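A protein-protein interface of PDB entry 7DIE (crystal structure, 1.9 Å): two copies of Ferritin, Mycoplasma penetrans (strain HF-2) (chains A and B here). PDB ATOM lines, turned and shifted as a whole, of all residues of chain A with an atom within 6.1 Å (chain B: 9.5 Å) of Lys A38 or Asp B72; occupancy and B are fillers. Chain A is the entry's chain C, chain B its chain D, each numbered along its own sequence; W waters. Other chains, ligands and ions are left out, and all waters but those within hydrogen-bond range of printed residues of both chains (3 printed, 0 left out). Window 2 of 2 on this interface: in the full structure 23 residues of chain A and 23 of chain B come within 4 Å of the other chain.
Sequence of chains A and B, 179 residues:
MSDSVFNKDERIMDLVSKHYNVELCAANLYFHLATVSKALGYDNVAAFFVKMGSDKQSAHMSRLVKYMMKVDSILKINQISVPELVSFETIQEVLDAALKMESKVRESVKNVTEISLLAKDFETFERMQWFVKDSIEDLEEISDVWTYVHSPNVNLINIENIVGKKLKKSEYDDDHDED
OG1 of Thr A35 is in hydrogen-bond range of N of Leu B75 (3.0 Å).
The side-chain hydroxyl of Ser B4 is in hydrogen-bond range of the side-chain carboxylate of Asp B72 (3.0 Å). O of Met B68 lies within hydrogen-bond range of N of Ser B73. The side-chain hydroxyl of Ser B73 lies close to the side-chain sulfur of Met B13, 3.8 Å away. The backbone carbonyl oxygen (O) of Val B71 is in hydrogen-bond range of the side-chain hydroxyl (OG) of Ser B73 (3.1 Å). NZ of Lys A38 lies within salt-bridge range of OD1 of Asp A43, at 3.2 Å.
Among the printed residues, merely in contact across the chains: Thr A35 with Ser B73, Lys A38 with Met B69, Thr A35 with Ile B74, Thr A35 with Val B65, Val A36 with Ile B74, Ala A39 with Asp B72, Lys A38 with Asp B72, Thr A35 with Met B69 and Ala A39 with Ile B74.
Of the printed residues of chain B, Thr A35 touches Val B65 (3.7 Å), Met B69 (3.97 Å), Ser B73 (3.4 Å), Ile B74 (3.6 Å) and Leu B75 (3.0 Å). Printed residues of chain B within 4 Å of Ala A39: Asp B72 (3.9 Å) and Ile B74 (3.997 Å). Ser B4 touches none of the printed residues of chain A. Leu B64 touches none of the printed residues of chain A. Of the printed residues of chain A, Val B65 touches Thr A35 (3.7 Å). Asp B72 touches just these residues of chain A: Lys A38 (3.9 Å) and Ala A39 (3.9 Å). Of the printed residues of chain A, Ser B73 touches Thr A35 (3.4 Å). Printed residues of chain A within 4 Å of Ile B74: Thr A35, Val A36 and Ala A39. The nearest residue of chain B that does not touch Lys A38 is Lys B70 (5.2 Å). The nearest printed residue of chain A that does not touch Ile B74 is Ser A37 (6.1 Å).
Of the 13 printed residues of chain A, 4 touch a printed residue of chain B. Printed residues of chain A that touch a printed residue of chain B: Thr A35, Val A36, Lys A38 and Ala A39. Hydrophobic or aromatic side chains of chain A within 4 Å of the printed part of chain B: Ala A39. Hydrophobic or aromatic side chains of chain B that line the printed part of chain A: Val B65, Met B69, Ile B74 and Leu B75. Among the printed residues, no Asp or Glu carboxylate lies within 4 Å of a Lys or Arg side-chain nitrogen of the other chain.
No position is printed for both chains. Of the 10 pairs that touch across the chains among the printed residues, none has its exchanged pair printed and touching as well.
Water W3 lies within hydrogen-bond range of O of Thr A35 and O of Ser B73. Water W2 bridges the backbone carbonyl oxygen (O) of Lys A38 (2.8 Å) and the side-chain carboxylate (OD1) of Asp B72 (3.1 Å). Water W1 lies within hydrogen-bond range of OD1 of Asp A43 (3.1 Å) and SD of Met B69 (3.7 Å).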
ATOM      1  N   LEU A  33      34.814  15.193  -8.020  1.00  0.00           N
ATOM      2  CA  LEU A  33      35.939  14.258  -8.037  1.00  0.00           C
ATOM      3  C   LEU A  33      35.562  12.903  -7.456  1.00  0.00           C
ATOM      4  O   LEU A  33      36.186  11.889  -7.793  1.00  0.00           O
ATOM      5  CB  LEU A  33      37.132  14.847  -7.280  1.00  0.00           C
ATOM      6  CG  LEU A  33      37.718  16.112  -7.907  1.00  0.00           C
ATOM      7  CD1 LEU A  33      38.933  16.607  -7.102  1.00  0.00           C
ATOM      8  CD2 LEU A  33      38.123  15.891  -9.373  1.00  0.00           C
ATOM      9  N   ALA A  34      34.563  12.859  -6.574  1.00  0.00           N
ATOM     10  CA  ALA A  34      34.075  11.564  -6.115  1.00  0.00           C
ATOM     11  C   ALA A  34      33.555  10.749  -7.289  1.00  0.00           C
ATOM     12  O   ALA A  34      33.912   9.579  -7.450  1.00  0.00           O
ATOM     13  CB  ALA A  34      32.988  11.755  -5.049  1.00  0.00           C
ATOM     14  N   THR A  35      32.729  11.360  -8.148  1.00  0.00           N
ATOM     15  CA  THR A  35      32.204  10.619  -9.295  1.00  0.00           C
ATOM     16  C   THR A  35      33.305  10.274 -10.298  1.00  0.00           C
ATOM     17  O   THR A  35      33.280   9.185 -10.879  1.00  0.00           O
ATOM     18  CB  THR A  35      31.056  11.403  -9.968  1.00  0.00           C
ATOM     19  OG1 THR A  35      31.549  12.624 -10.542  1.00  0.00           O
ATOM     20  CG2 THR A  35      29.948  11.719  -8.939  1.00  0.00           C
ATOM     21  N   VAL A  36      34.294  11.156 -10.490  1.00  0.00           N
ATOM     22  CA  VAL A  36      35.406  10.840 -11.390  1.00  0.00           C
ATOM     23  C   VAL A  36      36.232   9.691 -10.828  1.00  0.00           C
ATOM     24  O   VAL A  36      36.548   8.730 -11.539  1.00  0.00           O
ATOM     25  CB  VAL A  36      36.285  12.081 -11.645  1.00  0.00           C
ATOM     26  CG1 VAL A  36      37.516  11.716 -12.490  1.00  0.00           C
ATOM     27  CG2 VAL A  36      35.464  13.206 -12.319  1.00  0.00           C
ATOM     28  N   SER A  37      36.598   9.776  -9.544  1.00  0.00           N
ATOM     29  CA  SER A  37      37.355   8.701  -8.899  1.00  0.00           C
ATOM     30  C   SER A  37      36.642   7.366  -9.039  1.00  0.00           C
ATOM     31  O   SER A  37      37.263   6.346  -9.359  1.00  0.00           O
ATOM     32  CB  SER A  37      37.563   9.031  -7.410  1.00  0.00           C
ATOM     33  OG  SER A  37      38.337  10.214  -7.250  1.00  0.00           O
ATOM     34  N   LYS A  38      35.333   7.353  -8.772  1.00  0.00           N
ATOM     35  CA  LYS A  38      34.555   6.123  -8.890  1.00  0.00           C
ATOM     36  C   LYS A  38      34.645   5.554 -10.304  1.00  0.00           C
ATOM     37  O   LYS A  38      34.905   4.358 -10.496  1.00  0.00           O
ATOM     38  CB  LYS A  38      33.097   6.412  -8.510  1.00  0.00           C
ATOM     39  CG  LYS A  38      32.175   5.206  -8.551  1.00  0.00           C
ATOM     40  CD  LYS A  38      32.569   4.146  -7.533  1.00  0.00           C
ATOM     41  CE  LYS A  38      31.707   2.896  -7.666  1.00  0.00           C
ATOM     42  NZ  LYS A  38      32.473   1.676  -7.212  1.00  0.00           N
ATOM     43  N   ALA A  39      34.453   6.413 -11.310  1.00  0.00           N
ATOM     44  CA  ALA A  39      34.494   5.965 -12.703  1.00  0.00           C
ATOM     45  C   ALA A  39      35.879   5.468 -13.090  1.00  0.00           C
ATOM     46  O   ALA A  39      36.004   4.616 -13.983  1.00  0.00           O
ATOM     47  CB  ALA A  39      34.059   7.098 -13.635  1.00  0.00           C
ATOM     48  N   LEU A  40      36.925   5.968 -12.432  1.00  0.00           N
ATOM     49  CA  LEU A  40      38.277   5.470 -12.672  1.00  0.00           C
ATOM     50  C   LEU A  40      38.565   4.164 -11.939  1.00  0.00           C
ATOM     51  O   LEU A  40      39.650   3.594 -12.119  1.00  0.00           O
ATOM     52  CB  LEU A  40      39.310   6.528 -12.271  1.00  0.00           C
ATOM     53  CG  LEU A  40      39.386   7.747 -13.181  1.00  0.00           C
ATOM     54  CD1 LEU A  40      40.234   8.841 -12.531  1.00  0.00           C
ATOM     55  CD2 LEU A  40      39.966   7.348 -14.546  1.00  0.00           C
ATOM     56  N   GLY A  41      37.629   3.677 -11.131  1.00  0.00           N
ATOM     57  CA  GLY A  41      37.781   2.419 -10.436  1.00  0.00           C
ATOM     58  C   GLY A  41      38.132   2.524  -8.966  1.00  0.00           C
ATOM     59  O   GLY A  41      38.443   1.499  -8.349  1.00  0.00           O
ATOM     60  N   TYR A  42      38.082   3.718  -8.380  1.00  0.00           N
ATOM     61  CA  TYR A  42      38.593   3.951  -7.032  1.00  0.00           C
ATOM     62  C   TYR A  42      37.417   4.233  -6.097  1.00  0.00           C
ATOM     63  O   TYR A  42      37.116   5.383  -5.772  1.00  0.00           O
ATOM     64  CB  TYR A  42      39.596   5.101  -7.051  1.00  0.00           C
ATOM     65  CG  TYR A  42      40.888   4.761  -7.752  1.00  0.00           C
ATOM     66  CD1 TYR A  42      41.025   4.907  -9.139  1.00  0.00           C
ATOM     67  CD2 TYR A  42      41.972   4.285  -7.027  1.00  0.00           C
ATOM     68  CE1 TYR A  42      42.227   4.582  -9.771  1.00  0.00           C
ATOM     69  CE2 TYR A  42      43.166   3.971  -7.644  1.00  0.00           C
ATOM     70  CZ  TYR A  42      43.290   4.114  -9.008  1.00  0.00           C
ATOM     71  OH  TYR A  42      44.492   3.780  -9.591  1.00  0.00           O
ATOM     72  N   ASP A  43      36.766   3.155  -5.645  1.00  0.00           N
ATOM     73  CA  ASP A  43      35.605   3.265  -4.754  1.00  0.00           C
ATOM     74  C   ASP A  43      35.943   3.987  -3.449  1.00  0.00           C
ATOM     75  O   ASP A  43      35.148   4.809  -2.958  1.00  0.00           O
ATOM     76  CB  ASP A  43      35.057   1.857  -4.470  1.00  0.00           C
ATOM     77  CG  ASP A  43      33.806   1.862  -3.599  1.00  0.00           C
ATOM     78  OD1 ASP A  43      32.736   2.278  -4.092  1.00  0.00           O
ATOM     79  OD2 ASP A  43      33.884   1.425  -2.423  1.00  0.00           O
ATOM     80  N   VAL A  45      38.625   6.009  -2.745  1.00  0.00           N
ATOM     81  CA  VAL A  45      38.952   7.411  -3.007  1.00  0.00           C
ATOM     82  C   VAL A  45      37.680   8.219  -3.231  1.00  0.00           C
ATOM     83  O   VAL A  45      37.552   9.357  -2.757  1.00  0.00           O
ATOM     84  CB  VAL A  45      39.920   7.536  -4.199  1.00  0.00           C
ATOM     85  CG1 VAL A  45      40.238   9.017  -4.474  1.00  0.00           C
ATOM     86  CG2 VAL A  45      41.209   6.740  -3.941  1.00  0.00           C
ATOM     87  N   ALA A  46      36.711   7.641  -3.948  1.00  0.00           N
ATOM     88  CA  ALA A  46      35.432   8.326  -4.149  1.00  0.00           C
ATOM     89  C   ALA A  46      34.745   8.620  -2.815  1.00  0.00           C
ATOM     90  O   ALA A  46      34.270   9.737  -2.577  1.00  0.00           O
ATOM     91  CB  ALA A  46      34.522   7.482  -5.047  1.00  0.00           C
ATOM     92  N   SER B   4      31.912   1.996 -19.390  1.00  0.00           N
ATOM     93  CA  SER B   4      31.408   1.361 -18.174  1.00  0.00           C
ATOM     94  C   SER B   4      30.416   0.242 -18.490  1.00  0.00           C
ATOM     95  O   SER B   4      29.691   0.297 -19.477  1.00  0.00           O
ATOM     96  CB  SER B   4      30.748   2.397 -17.254  1.00  0.00           C
ATOM     97  OG  SER B   4      30.031   1.771 -16.200  1.00  0.00           O
ATOM     98  N   VAL B   5      30.383  -0.778 -17.629  1.00  0.00           N
ATOM     99  CA  VAL B   5      29.425  -1.859 -17.809  1.00  0.00           C
ATOM    100  C   VAL B   5      27.986  -1.383 -17.632  1.00  0.00           C
ATOM    101  O   VAL B   5      27.049  -2.057 -18.078  1.00  0.00           O
ATOM    102  CB  VAL B   5      29.789  -3.017 -16.854  1.00  0.00           C
ATOM    103  CG1 VAL B   5      31.285  -3.303 -16.945  1.00  0.00           C
ATOM    104  CG2 VAL B   5      29.425  -2.692 -15.416  1.00  0.00           C
ATOM    105  N   PHE B   6      27.774  -0.219 -17.014  1.00  0.00           N
ATOM    106  CA  PHE B   6      26.406   0.241 -16.785  1.00  0.00           C
ATOM    107  C   PHE B   6      25.809   0.910 -18.013  1.00  0.00           C
ATOM    108  O   PHE B   6      24.593   0.815 -18.237  1.00  0.00           O
ATOM    109  CB  PHE B   6      26.380   1.178 -15.586  1.00  0.00           C
ATOM    110  CG  PHE B   6      26.608   0.453 -14.287  1.00  0.00           C
ATOM    111  CD1 PHE B   6      25.544  -0.156 -13.626  1.00  0.00           C
ATOM    112  CD2 PHE B   6      27.885   0.321 -13.768  1.00  0.00           C
ATOM    113  CE1 PHE B   6      25.745  -0.858 -12.436  1.00  0.00           C
ATOM    114  CE2 PHE B   6      28.094  -0.392 -12.571  1.00  0.00           C
ATOM    115  CZ  PHE B   6      27.020  -0.967 -11.911  1.00  0.00           C
ATOM    116  N   ASN B   7      26.637   1.596 -18.798  1.00  0.00           N
ATOM    117  CA  ASN B   7      26.230   2.073 -20.114  1.00  0.00           C
ATOM    118  C   ASN B   7      24.978   2.945 -20.013  1.00  0.00           C
ATOM    119  O   ASN B   7      23.978   2.726 -20.703  1.00  0.00           O
ATOM    120  CB  ASN B   7      26.004   0.885 -21.048  1.00  0.00           C
ATOM    121  CG  ASN B   7      25.870   1.293 -22.486  1.00  0.00           C
ATOM    122  OD1 ASN B   7      26.502   2.253 -22.933  1.00  0.00           O
ATOM    123  ND2 ASN B   7      25.056   0.555 -23.235  1.00  0.00           N
ATOM    124  N   LYS B   8      25.017   3.901 -19.090  1.00  0.00           N
ATOM    125  CA  LYS B   8      23.905   4.823 -18.940  1.00  0.00           C
ATOM    126  C   LYS B   8      23.911   5.821 -20.097  1.00  0.00           C
ATOM    127  O   LYS B   8      24.951   6.099 -20.694  1.00  0.00           O
ATOM    128  CB  LYS B   8      24.006   5.563 -17.602  1.00  0.00           C
ATOM    129  CG  LYS B   8      24.133   4.625 -16.368  1.00  0.00           C
ATOM    130  CD  LYS B   8      22.980   3.661 -16.277  1.00  0.00           C
ATOM    131  CE  LYS B   8      21.670   4.379 -15.950  1.00  0.00           C
ATOM    132  NZ  LYS B   8      20.512   3.410 -16.035  1.00  0.00           N
ATOM    133  N   GLU B  10      24.001   9.345 -21.688  1.00  0.00           N
ATOM    134  CA  GLU B  10      24.582  10.607 -21.250  1.00  0.00           C
ATOM    135  C   GLU B  10      23.552  11.716 -21.100  1.00  0.00           C
ATOM    136  O   GLU B  10      23.705  12.571 -20.222  1.00  0.00           O
ATOM    137  CB  GLU B  10      25.687  11.045 -22.219  1.00  0.00           C
ATOM    138  CG  GLU B  10      26.668  12.042 -21.606  1.00  0.00           C
ATOM    139  CD  GLU B  10      27.943  12.206 -22.422  1.00  0.00           C
ATOM    140  OE1 GLU B  10      28.043  13.198 -23.180  1.00  0.00           O
ATOM    141  OE2 GLU B  10      28.843  11.346 -22.302  1.00  0.00           O
ATOM    142  N   MET B  13      21.826  11.031 -17.750  1.00  0.00           N
ATOM    143  CA  MET B  13      22.718  11.323 -16.627  1.00  0.00           C
ATOM    144  C   MET B  13      23.025  12.815 -16.538  1.00  0.00           C
ATOM    145  O   MET B  13      23.151  13.349 -15.434  1.00  0.00           O
ATOM    146  CB  MET B  13      23.998  10.496 -16.728  1.00  0.00           C
ATOM    147  CG  MET B  13      23.754   8.980 -16.671  1.00  0.00           C
ATOM    148  SD  MET B  13      22.854   8.426 -15.190  1.00  0.00           S
ATOM    149  CE  MET B  13      21.255   8.097 -15.795  1.00  0.00           C
ATOM    150  N   LEU B  64      21.623  11.833  -4.892  1.00  0.00           N
ATOM    151  CA  LEU B  64      21.904  11.972  -6.323  1.00  0.00           C
ATOM    152  C   LEU B  64      23.356  11.627  -6.634  1.00  0.00           C
ATOM    153  O   LEU B  64      23.636  10.857  -7.556  1.00  0.00           O
ATOM    154  CB  LEU B  64      21.566  13.391  -6.804  1.00  0.00           C
ATOM    155  CG  LEU B  64      20.079  13.784  -6.737  1.00  0.00           C
ATOM    156  CD1 LEU B  64      19.872  15.303  -6.792  1.00  0.00           C
ATOM    157  CD2 LEU B  64      19.264  13.114  -7.855  1.00  0.00           C
ATOM    158  N   VAL B  65      24.301  12.157  -5.861  1.00  0.00           N
ATOM    159  CA  VAL B  65      25.689  11.807  -6.141  1.00  0.00           C
ATOM    160  C   VAL B  65      25.943  10.320  -5.875  1.00  0.00           C
ATOM    161  O   VAL B  65      26.704   9.677  -6.606  1.00  0.00           O
ATOM    162  CB  VAL B  65      26.655  12.733  -5.372  1.00  0.00           C
ATOM    163  CG1 VAL B  65      26.622  12.469  -3.879  1.00  0.00           C
ATOM    164  CG2 VAL B  65      28.071  12.556  -5.913  1.00  0.00           C
ATOM    165  N   LYS B  66      25.284   9.745  -4.862  1.00  0.00           N
ATOM    166  CA  LYS B  66      25.447   8.319  -4.584  1.00  0.00           C
ATOM    167  C   LYS B  66      24.929   7.474  -5.736  1.00  0.00           C
ATOM    168  O   LYS B  66      25.550   6.472  -6.112  1.00  0.00           O
ATOM    169  CB  LYS B  66      24.721   7.946  -3.291  1.00  0.00           C
ATOM    170  CG  LYS B  66      24.568   6.455  -3.069  1.00  0.00           C
ATOM    171  CD  LYS B  66      24.045   6.122  -1.663  1.00  0.00           C
ATOM    172  CE  LYS B  66      24.073   4.615  -1.426  1.00  0.00           C
ATOM    173  NZ  LYS B  66      23.485   4.235  -0.124  1.00  0.00           N
ATOM    174  N   TYR B  67      23.794   7.869  -6.314  1.00  0.00           N
ATOM    175  CA  TYR B  67      23.261   7.159  -7.468  1.00  0.00           C
ATOM    176  C   TYR B  67      24.200   7.272  -8.668  1.00  0.00           C
ATOM    177  O   TYR B  67      24.483   6.277  -9.342  1.00  0.00           O
ATOM    178  CB  TYR B  67      21.873   7.693  -7.822  1.00  0.00           C
ATOM    179  CG  TYR B  67      21.363   7.096  -9.110  1.00  0.00           C
ATOM    180  CD1 TYR B  67      21.090   5.736  -9.197  1.00  0.00           C
ATOM    181  CD2 TYR B  67      21.186   7.883 -10.258  1.00  0.00           C
ATOM    182  CE1 TYR B  67      20.639   5.162 -10.385  1.00  0.00           C
ATOM    183  CE2 TYR B  67      20.740   7.308 -11.458  1.00  0.00           C
ATOM    184  CZ  TYR B  67      20.467   5.954 -11.506  1.00  0.00           C
ATOM    185  OH  TYR B  67      20.038   5.375 -12.676  1.00  0.00           O
ATOM    186  N   MET B  68      24.697   8.483  -8.956  1.00  0.00           N
ATOM    187  CA  MET B  68      25.586   8.622 -10.105  1.00  0.00           C
ATOM    188  C   MET B  68      26.808   7.733  -9.962  1.00  0.00           C
ATOM    189  O   MET B  68      27.227   7.078 -10.925  1.00  0.00           O
ATOM    190  CB  MET B  68      25.982  10.087 -10.292  1.00  0.00           C
ATOM    191  CG  MET B  68      24.765  10.947 -10.596  1.00  0.00           C
ATOM    192  SD  MET B  68      25.171  12.568 -11.261  1.00  0.00           S
ATOM    193  CE  MET B  68      25.461  12.108 -12.966  1.00  0.00           C
ATOM    194  N   MET B  69      27.360   7.648  -8.748  1.00  0.00           N
ATOM    195  CA  MET B  69      28.501   6.763  -8.516  1.00  0.00           C
ATOM    196  C   MET B  69      28.125   5.297  -8.720  1.00  0.00           C
ATOM    197  O   MET B  69      28.923   4.519  -9.251  1.00  0.00           O
ATOM    198  CB  MET B  69      29.043   6.995  -7.103  1.00  0.00           C
ATOM    199  CG  MET B  69      29.904   8.265  -6.976  1.00  0.00           C
ATOM    200  SD  MET B  69      30.599   8.449  -5.312  1.00  0.00           S
ATOM    201  CE  MET B  69      29.113   8.727  -4.380  1.00  0.00           C
ATOM    202  N   LYS B  70      26.907   4.901  -8.317  1.00  0.00           N
ATOM    203  CA  LYS B  70      26.491   3.507  -8.512  1.00  0.00           C
ATOM    204  C   LYS B  70      26.569   3.110  -9.980  1.00  0.00           C
ATOM    205  O   LYS B  70      26.927   1.970 -10.304  1.00  0.00           O
ATOM    206  CB  LYS B  70      25.068   3.284  -7.996  1.00  0.00           C
ATOM    207  CG  LYS B  70      24.929   3.226  -6.478  1.00  0.00           C
ATOM    208  CD  LYS B  70      25.438   1.900  -5.904  1.00  0.00           C
ATOM    209  CE  LYS B  70      25.486   1.950  -4.375  1.00  0.00           C
ATOM    210  NZ  LYS B  70      26.344   0.859  -3.825  1.00  0.00           N
ATOM    211  N   VAL B  71      26.234   4.034 -10.880  1.00  0.00           N
ATOM    212  CA  VAL B  71      26.212   3.754 -12.315  1.00  0.00           C
ATOM    213  C   VAL B  71      27.388   4.415 -13.040  1.00  0.00           C
ATOM    214  O   VAL B  71      27.328   4.640 -14.258  1.00  0.00           O
ATOM    215  CB  VAL B  71      24.859   4.145 -12.934  1.00  0.00           C
ATOM    216  CG1 VAL B  71      23.761   3.237 -12.369  1.00  0.00           C
ATOM    217  CG2 VAL B  71      24.538   5.622 -12.671  1.00  0.00           C
ATOM    218  N   ASP B  72      28.456   4.728 -12.307  1.00  0.00           N
ATOM    219  CA  ASP B  72      29.730   5.185 -12.867  1.00  0.00           C
ATOM    220  C   ASP B  72      29.592   6.455 -13.703  1.00  0.00           C
ATOM    221  O   ASP B  72      30.362   6.655 -14.642  1.00  0.00           O
ATOM    222  CB  ASP B  72      30.400   4.095 -13.723  1.00  0.00           C
ATOM    223  CG  ASP B  72      30.965   2.948 -12.903  1.00  0.00           C
ATOM    224  OD1 ASP B  72      31.053   3.059 -11.663  1.00  0.00           O
ATOM    225  OD2 ASP B  72      31.325   1.921 -13.512  1.00  0.00           O
ATOM    226  N   SER B  73      28.634   7.331 -13.402  1.00  0.00           N
ATOM    227  CA  SER B  73      28.467   8.558 -14.182  1.00  0.00           C
ATOM    228  C   SER B  73      28.969   9.778 -13.420  1.00  0.00           C
ATOM    229  O   SER B  73      29.155   9.743 -12.200  1.00  0.00           O
ATOM    230  CB  SER B  73      27.001   8.749 -14.602  1.00  0.00           C
ATOM    231  OG  SER B  73      26.496   7.515 -15.074  1.00  0.00           O
ATOM    232  N   ILE B  74      29.155  10.879 -14.158  1.00  0.00           N
ATOM    233  CA  ILE B  74      29.920  12.035 -13.690  1.00  0.00           C
ATOM    234  C   ILE B  74      28.977  13.159 -13.291  1.00  0.00           C
ATOM    235  O   ILE B  74      28.109  13.577 -14.075  1.00  0.00           O
ATOM    236  CB  ILE B  74      30.915  12.523 -14.763  1.00  0.00           C
ATOM    237  CG1 ILE B  74      31.834  11.386 -15.208  1.00  0.00           C
ATOM    238  CG2 ILE B  74      31.761  13.679 -14.219  1.00  0.00           C
ATOM    239  CD1 ILE B  74      32.668  10.815 -14.106  1.00  0.00           C
ATOM    240  N   LEU B  75      29.163  13.679 -12.083  1.00  0.00           N
ATOM    241  CA  LEU B  75      28.421  14.853 -11.634  1.00  0.00           C
ATOM    242  C   LEU B  75      29.161  16.116 -12.054  1.00  0.00           C
ATOM    243  O   LEU B  75      30.352  16.268 -11.757  1.00  0.00           O
ATOM    244  CB  LEU B  75      28.244  14.838 -10.109  1.00  0.00           C
ATOM    245  CG  LEU B  75      27.714  16.110  -9.443  1.00  0.00           C
ATOM    246  CD1 LEU B  75      26.288  16.360  -9.882  1.00  0.00           C
ATOM    247  CD2 LEU B  75      27.791  15.996  -7.895  1.00  0.00           C
ATOM    248  N   GLU B 123      16.277   2.326 -14.010  1.00  0.00           N
ATOM    249  CA  GLU B 123      17.116   2.580 -12.847  1.00  0.00           C
ATOM    250  C   GLU B 123      16.984   4.024 -12.391  1.00  0.00           C
ATOM    251  O   GLU B 123      16.839   4.295 -11.196  1.00  0.00           O
ATOM    252  CB  GLU B 123      18.575   2.232 -13.163  1.00  0.00           C
ATOM    253  CG  GLU B 123      18.758   0.710 -13.386  1.00  0.00           C
ATOM    254  CD  GLU B 123      20.136   0.320 -13.909  1.00  0.00           C
ATOM    255  OE1 GLU B 123      20.912   1.215 -14.327  1.00  0.00           O
ATOM    256  OE2 GLU B 123      20.436  -0.899 -13.921  1.00  0.00           O
HETATM  257  O   HOH W   1      31.214   4.847  -4.820  1.00  0.00           O
HETATM  258  O   HOH W   2      33.751   1.802 -10.957  1.00  0.00           O
HETATM  259  O   HOH W   3      30.869   7.779 -10.833  1.00  0.00           O
